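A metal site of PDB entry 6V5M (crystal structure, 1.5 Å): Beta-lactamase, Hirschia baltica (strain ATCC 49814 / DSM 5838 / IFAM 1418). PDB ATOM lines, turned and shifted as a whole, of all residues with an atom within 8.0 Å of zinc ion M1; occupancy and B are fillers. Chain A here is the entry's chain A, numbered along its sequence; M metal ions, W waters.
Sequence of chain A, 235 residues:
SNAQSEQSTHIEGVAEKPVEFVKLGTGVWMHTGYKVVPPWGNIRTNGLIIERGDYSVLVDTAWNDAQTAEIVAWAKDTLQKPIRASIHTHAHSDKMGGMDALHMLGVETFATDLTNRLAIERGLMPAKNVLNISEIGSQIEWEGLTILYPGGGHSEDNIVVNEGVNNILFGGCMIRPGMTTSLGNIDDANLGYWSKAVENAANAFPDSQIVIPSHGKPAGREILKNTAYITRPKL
Zinc ion M1 is bound by water W1, ND1 of His 92, NE2 of His 154 and NE2 of His 90. Zinc ion M1 has four donor atoms within binding distance.
OD1 of Asp 94 touches zinc ion M1, at 3.9 Å. Four residues have an atom within 4 Å of zinc ion M1: His 90, His 92, Asp 94 and His 154. The nearest printed residue that does not touch zinc ion M1 is Cys 173 (4.01 Å).
A ring nitrogen (NE2) of His 92 sits at hydrogen-bond distance from the side-chain carboxylate of Asp 188. The backbone carbonyl oxygen (O) of Asn 185 sits close to a ring nitrogen (ND1) of His 154, at 3.5 Å. N of His 154 lies within hydrogen-bond range of OD1 of Asn 158, 2.8 Å away.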
ATOM      1  N   TRP A  63       2.658  -6.730  -0.483  1.00  0.00           N
ATOM      2  CA  TRP A  63       1.387  -6.215  -1.000  1.00  0.00           C
ATOM      3  C   TRP A  63       1.338  -6.142  -2.522  1.00  0.00           C
ATOM      4  O   TRP A  63       0.233  -6.130  -3.088  1.00  0.00           O
ATOM      5  CB  TRP A  63       1.143  -4.814  -0.456  1.00  0.00           C
ATOM      6  CG  TRP A  63       0.871  -4.735   0.990  1.00  0.00           C
ATOM      7  CD1 TRP A  63       1.728  -4.279   1.971  1.00  0.00           C
ATOM      8  CD2 TRP A  63      -0.379  -4.995   1.646  1.00  0.00           C
ATOM      9  NE1 TRP A  63       1.095  -4.278   3.198  1.00  0.00           N
ATOM     10  CE2 TRP A  63      -0.191  -4.718   3.032  1.00  0.00           C
ATOM     11  CE3 TRP A  63      -1.623  -5.465   1.220  1.00  0.00           C
ATOM     12  CZ2 TRP A  63      -1.212  -4.884   3.983  1.00  0.00           C
ATOM     13  CZ3 TRP A  63      -2.671  -5.607   2.191  1.00  0.00           C
ATOM     14  CH2 TRP A  63      -2.442  -5.319   3.539  1.00  0.00           C
ATOM     15  N   THR A  89      -0.175 -18.288   1.965  1.00  0.00           N
ATOM     16  CA  THR A  89      -0.937 -18.800   3.110  1.00  0.00           C
ATOM     17  C   THR A  89      -2.433 -18.483   3.074  1.00  0.00           C
ATOM     18  O   THR A  89      -3.175 -19.088   3.864  1.00  0.00           O
ATOM     19  CB  THR A  89      -0.299 -18.371   4.451  1.00  0.00           C
ATOM     20  OG1 THR A  89      -0.271 -16.937   4.567  1.00  0.00           O
ATOM     21  CG2 THR A  89       1.137 -18.974   4.579  1.00  0.00           C
ATOM     22  N   HIS A  90      -2.906 -17.642   2.146  1.00  0.00           N
ATOM     23  CA  HIS A  90      -4.316 -17.598   1.740  1.00  0.00           C
ATOM     24  C   HIS A  90      -4.438 -16.581   0.605  1.00  0.00           C
ATOM     25  O   HIS A  90      -3.500 -15.835   0.302  1.00  0.00           O
ATOM     26  CB  HIS A  90      -5.299 -17.278   2.878  1.00  0.00           C
ATOM     27  CG  HIS A  90      -5.169 -15.887   3.397  1.00  0.00           C
ATOM     28  ND1 HIS A  90      -4.198 -15.545   4.317  1.00  0.00           N
ATOM     29  CD2 HIS A  90      -5.891 -14.766   3.175  1.00  0.00           C
ATOM     30  CE1 HIS A  90      -4.330 -14.262   4.639  1.00  0.00           C
ATOM     31  NE2 HIS A  90      -5.329 -13.765   3.942  1.00  0.00           N
ATOM     32  N   ALA A  91      -5.627 -16.556  -0.004  1.00  0.00           N
ATOM     33  CA  ALA A  91      -5.851 -15.747  -1.204  1.00  0.00           C
ATOM     34  C   ALA A  91      -6.334 -14.334  -0.850  1.00  0.00           C
ATOM     35  O   ALA A  91      -7.494 -13.971  -1.029  1.00  0.00           O
ATOM     36  CB  ALA A  91      -6.845 -16.455  -2.134  1.00  0.00           C
ATOM     37  N   HIS A  92      -5.424 -13.526  -0.339  1.00  0.00           N
ATOM     38  CA  HIS A  92      -5.643 -12.091  -0.213  1.00  0.00           C
ATOM     39  C   HIS A  92      -4.409 -11.367  -0.726  1.00  0.00           C
ATOM     40  O   HIS A  92      -3.329 -11.974  -0.863  1.00  0.00           O
ATOM     41  CB  HIS A  92      -5.926 -11.623   1.232  1.00  0.00           C
ATOM     42  CG  HIS A  92      -7.328 -11.850   1.684  1.00  0.00           C
ATOM     43  ND1 HIS A  92      -7.661 -11.967   3.027  1.00  0.00           N
ATOM     44  CD2 HIS A  92      -8.488 -11.970   0.998  1.00  0.00           C
ATOM     45  CE1 HIS A  92      -8.970 -12.115   3.135  1.00  0.00           C
ATOM     46  NE2 HIS A  92      -9.501 -12.122   1.931  1.00  0.00           N
ATOM     47  N   SER A  93      -4.563 -10.075  -0.996  1.00  0.00           N
ATOM     48  CA  SER A  93      -3.510  -9.325  -1.705  1.00  0.00           C
ATOM     49  C   SER A  93      -2.267  -9.079  -0.839  1.00  0.00           C
ATOM     50  O   SER A  93      -1.198  -8.775  -1.390  1.00  0.00           O
ATOM     51  CB  SER A  93      -4.068  -8.007  -2.241  1.00  0.00           C
ATOM     52  OG  SER A  93      -4.371  -7.115  -1.185  1.00  0.00           O
ATOM     53  N   ASP A  94      -2.366  -9.179   0.485  1.00  0.00           N
ATOM     54  CA  ASP A  94      -1.152  -9.092   1.281  1.00  0.00           C
ATOM     55  C   ASP A  94      -0.261 -10.322   1.153  1.00  0.00           C
ATOM     56  O   ASP A  94       0.931 -10.251   1.457  1.00  0.00           O
ATOM     57  CB  ASP A  94      -1.409  -8.743   2.762  1.00  0.00           C
ATOM     58  CG  ASP A  94      -2.542  -9.572   3.413  1.00  0.00           C
ATOM     59  OD1 ASP A  94      -3.418 -10.149   2.756  1.00  0.00           O
ATOM     60  OD2 ASP A  94      -2.566  -9.578   4.645  1.00  0.00           O
ATOM     61  N   LYS A  95      -0.833 -11.443   0.731  1.00  0.00           N
ATOM     62  CA  LYS A  95      -0.129 -12.720   0.643  1.00  0.00           C
ATOM     63  C   LYS A  95       0.190 -13.129  -0.778  1.00  0.00           C
ATOM     64  O   LYS A  95       1.123 -13.913  -0.991  1.00  0.00           O
ATOM     65  CB  LYS A  95      -0.988 -13.833   1.301  1.00  0.00           C
ATOM     66  CG  LYS A  95      -1.633 -13.471   2.667  1.00  0.00           C
ATOM     67  CD  LYS A  95      -0.683 -13.619   3.871  1.00  0.00           C
ATOM     68  CE  LYS A  95       0.226 -12.384   4.023  1.00  0.00           C
ATOM     69  NZ  LYS A  95       1.266 -12.700   5.062  1.00  0.00           N
ATOM     70  N   ARG A 122     -10.987 -13.865  -6.640  1.00  0.00           N
ATOM     71  CA  ARG A 122     -10.741 -12.609  -5.943  1.00  0.00           C
ATOM     72  C   ARG A 122      -9.890 -11.647  -6.740  1.00  0.00           C
ATOM     73  O   ARG A 122      -9.512 -10.598  -6.219  1.00  0.00           O
ATOM     74  CB  ARG A 122     -10.115 -12.864  -4.568  1.00  0.00           C
ATOM     75  CG  ARG A 122     -11.060 -13.598  -3.613  1.00  0.00           C
ATOM     76  CD  ARG A 122     -10.421 -13.982  -2.283  1.00  0.00           C
ATOM     77  NE  ARG A 122     -11.377 -14.763  -1.502  1.00  0.00           N
ATOM     78  CZ  ARG A 122     -11.117 -15.336  -0.328  1.00  0.00           C
ATOM     79  NH1 ARG A 122      -9.905 -15.228   0.219  1.00  0.00           N
ATOM     80  NH2 ARG A 122     -12.073 -16.038   0.297  1.00  0.00           N
ATOM     81  N   HIS A 154      -9.418 -16.850   9.525  1.00  0.00           N
ATOM     82  CA  HIS A 154      -9.410 -15.544   8.882  1.00  0.00           C
ATOM     83  C   HIS A 154      -9.928 -15.641   7.452  1.00  0.00           C
ATOM     84  O   HIS A 154     -10.631 -14.751   6.958  1.00  0.00           O
ATOM     85  CB  HIS A 154      -7.969 -15.027   8.878  1.00  0.00           C
ATOM     86  CG  HIS A 154      -7.743 -13.912   7.913  1.00  0.00           C
ATOM     87  ND1 HIS A 154      -8.067 -12.592   8.199  1.00  0.00           N
ATOM     88  CD2 HIS A 154      -7.281 -13.921   6.639  1.00  0.00           C
ATOM     89  CE1 HIS A 154      -7.751 -11.833   7.159  1.00  0.00           C
ATOM     90  NE2 HIS A 154      -7.274 -12.613   6.196  1.00  0.00           N
ATOM     91  N   SER A 155      -9.548 -16.713   6.741  1.00  0.00           N
ATOM     92  CA  SER A 155     -10.077 -17.044   5.419  1.00  0.00           C
ATOM     93  C   SER A 155     -10.265 -18.562   5.392  1.00  0.00           C
ATOM     94  O   SER A 155      -9.560 -19.296   6.105  1.00  0.00           O
ATOM     95  CB  SER A 155      -9.077 -16.549   4.343  1.00  0.00           C
ATOM     96  OG  SER A 155      -9.560 -16.683   3.014  1.00  0.00           O
ATOM     97  N   ASP A 157      -9.398 -20.741   3.451  1.00  0.00           N
ATOM     98  CA  ASP A 157      -8.265 -21.473   2.918  1.00  0.00           C
ATOM     99  C   ASP A 157      -6.999 -21.271   3.743  1.00  0.00           C
ATOM    100  O   ASP A 157      -5.942 -21.759   3.330  1.00  0.00           O
ATOM    101  CB  ASP A 157      -7.974 -21.032   1.470  1.00  0.00           C
ATOM    102  CG  ASP A 157      -7.702 -19.529   1.349  1.00  0.00           C
ATOM    103  OD1 ASP A 157      -8.370 -18.712   2.045  1.00  0.00           O
ATOM    104  OD2 ASP A 157      -6.849 -19.163   0.511  1.00  0.00           O
ATOM    105  N   ASN A 158      -7.056 -20.560   4.870  1.00  0.00           N
ATOM    106  CA  ASN A 158      -5.819 -20.205   5.561  1.00  0.00           C
ATOM    107  C   ASN A 158      -5.019 -21.440   5.991  1.00  0.00           C
ATOM    108  O   ASN A 158      -5.565 -22.409   6.519  1.00  0.00           O
ATOM    109  CB  ASN A 158      -5.980 -19.148   6.671  1.00  0.00           C
ATOM    110  CG  ASN A 158      -6.962 -19.518   7.824  1.00  0.00           C
ATOM    111  OD1 ASN A 158      -7.492 -18.612   8.451  1.00  0.00           O
ATOM    112  ND2 ASN A 158      -7.240 -20.799   8.027  1.00  0.00           N
ATOM    113  N   GLY A 172       0.505 -16.274   9.955  1.00  0.00           N
ATOM    114  CA  GLY A 172      -0.148 -15.473   8.928  1.00  0.00           C
ATOM    115  C   GLY A 172      -1.313 -14.658   9.493  1.00  0.00           C
ATOM    116  O   GLY A 172      -1.294 -14.228  10.649  1.00  0.00           O
ATOM    117  N   CYS A 173      -2.333 -14.469   8.659  1.00  0.00           N
ATOM    118  CA  CYS A 173      -3.454 -13.626   9.048  1.00  0.00           C
ATOM    119  C   CYS A 173      -4.429 -14.355   9.961  1.00  0.00           C
ATOM    120  O   CYS A 173      -5.291 -13.694  10.562  1.00  0.00           O
ATOM    121  CB  CYS A 173      -4.186 -13.093   7.812  1.00  0.00           C
ATOM    122  SG  CYS A 173      -3.010 -12.186   6.786  1.00  0.00           S
ATOM    123  N   MET A 174      -4.292 -15.688  10.128  1.00  0.00           N
ATOM    124  CA  MET A 174      -5.119 -16.404  11.089  1.00  0.00           C
ATOM    125  C   MET A 174      -4.771 -16.029  12.526  1.00  0.00           C
ATOM    126  O   MET A 174      -5.613 -16.199  13.414  1.00  0.00           O
ATOM    127  CB  MET A 174      -4.947 -17.919  10.877  1.00  0.00           C
ATOM    128  CG  MET A 174      -6.034 -18.779  11.569  1.00  0.00           C
ATOM    129  SD  MET A 174      -5.730 -20.511  11.391  1.00  0.00           S
ATOM    130  CE  MET A 174      -4.606 -20.696  12.771  1.00  0.00           C
ATOM    131  N   ASN A 185      -9.752  -7.742   8.763  1.00  0.00           N
ATOM    132  CA  ASN A 185     -10.617  -7.956   7.613  1.00  0.00           C
ATOM    133  C   ASN A 185     -11.305  -9.313   7.735  1.00  0.00           C
ATOM    134  O   ASN A 185     -10.680 -10.368   7.545  1.00  0.00           O
ATOM    135  CB  ASN A 185      -9.808  -7.900   6.317  1.00  0.00           C
ATOM    136  CG  ASN A 185     -10.610  -8.323   5.119  1.00  0.00           C
ATOM    137  OD1 ASN A 185     -11.844  -8.295   5.150  1.00  0.00           O
ATOM    138  ND2 ASN A 185      -9.927  -8.741   4.063  1.00  0.00           N
ATOM    139  N   ILE A 186     -12.603  -9.291   8.023  1.00  0.00           N
ATOM    140  CA  ILE A 186     -13.357 -10.524   8.228  1.00  0.00           C
ATOM    141  C   ILE A 186     -14.283 -10.824   7.052  1.00  0.00           C
ATOM    142  O   ILE A 186     -15.144 -11.718   7.170  1.00  0.00           O
ATOM    143  CB  ILE A 186     -14.128 -10.531   9.559  1.00  0.00           C
ATOM    144  CG1 ILE A 186     -15.174  -9.407   9.604  1.00  0.00           C
ATOM    145  CG2 ILE A 186     -13.164 -10.520  10.742  1.00  0.00           C
ATOM    146  CD1 ILE A 186     -16.153  -9.609  10.696  1.00  0.00           C
ATOM    147  N   ASP A 188     -13.995 -12.510   4.481  1.00  0.00           N
ATOM    148  CA  ASP A 188     -13.895 -13.888   4.022  1.00  0.00           C
ATOM    149  C   ASP A 188     -13.730 -14.875   5.190  1.00  0.00           C
ATOM    150  O   ASP A 188     -13.357 -16.032   4.975  1.00  0.00           O
ATOM    151  CB  ASP A 188     -12.762 -14.002   3.001  1.00  0.00           C
ATOM    152  CG  ASP A 188     -13.035 -13.181   1.729  1.00  0.00           C
ATOM    153  OD1 ASP A 188     -14.205 -13.218   1.238  1.00  0.00           O
ATOM    154  OD2 ASP A 188     -12.106 -12.480   1.223  1.00  0.00           O
ATOM    155  N   SER A 214       0.679 -11.919  10.530  1.00  0.00           N
ATOM    156  CA  SER A 214       0.944 -11.083   9.342  1.00  0.00           C
ATOM    157  C   SER A 214       1.009  -9.599   9.692  1.00  0.00           C
ATOM    158  O   SER A 214       1.790  -8.858   9.092  1.00  0.00           O
ATOM    159  CB  SER A 214      -0.148 -11.233   8.297  1.00  0.00           C
ATOM    160  OG  SER A 214      -0.053 -12.472   7.675  1.00  0.00           O
ATOM    161  N   HIS A 215       0.167  -9.132  10.624  1.00  0.00           N
ATOM    162  CA  HIS A 215      -0.065  -7.691  10.769  1.00  0.00           C
ATOM    163  C   HIS A 215       0.407  -7.127  12.101  1.00  0.00           C
ATOM    164  O   HIS A 215      -0.086  -6.081  12.536  1.00  0.00           O
ATOM    165  CB  HIS A 215      -1.531  -7.355  10.466  1.00  0.00           C
ATOM    166  CG  HIS A 215      -1.950  -7.792   9.103  1.00  0.00           C
ATOM    167  ND1 HIS A 215      -1.314  -7.352   7.959  1.00  0.00           N
ATOM    168  CD2 HIS A 215      -2.890  -8.674   8.707  1.00  0.00           C
ATOM    169  CE1 HIS A 215      -1.883  -7.920   6.904  1.00  0.00           C
ATOM    170  NE2 HIS A 215      -2.841  -8.738   7.323  1.00  0.00           N
HETATM  171 ZN    ZN M   1      -6.307 -12.060   4.511  1.00  0.00          ZN
HETATM  172 ZN    ZN M   2      -3.909 -10.125   6.204  1.00  0.00          ZN
HETATM  173  O   HOH W   1      -5.348 -10.375   4.779  1.00  0.00           O
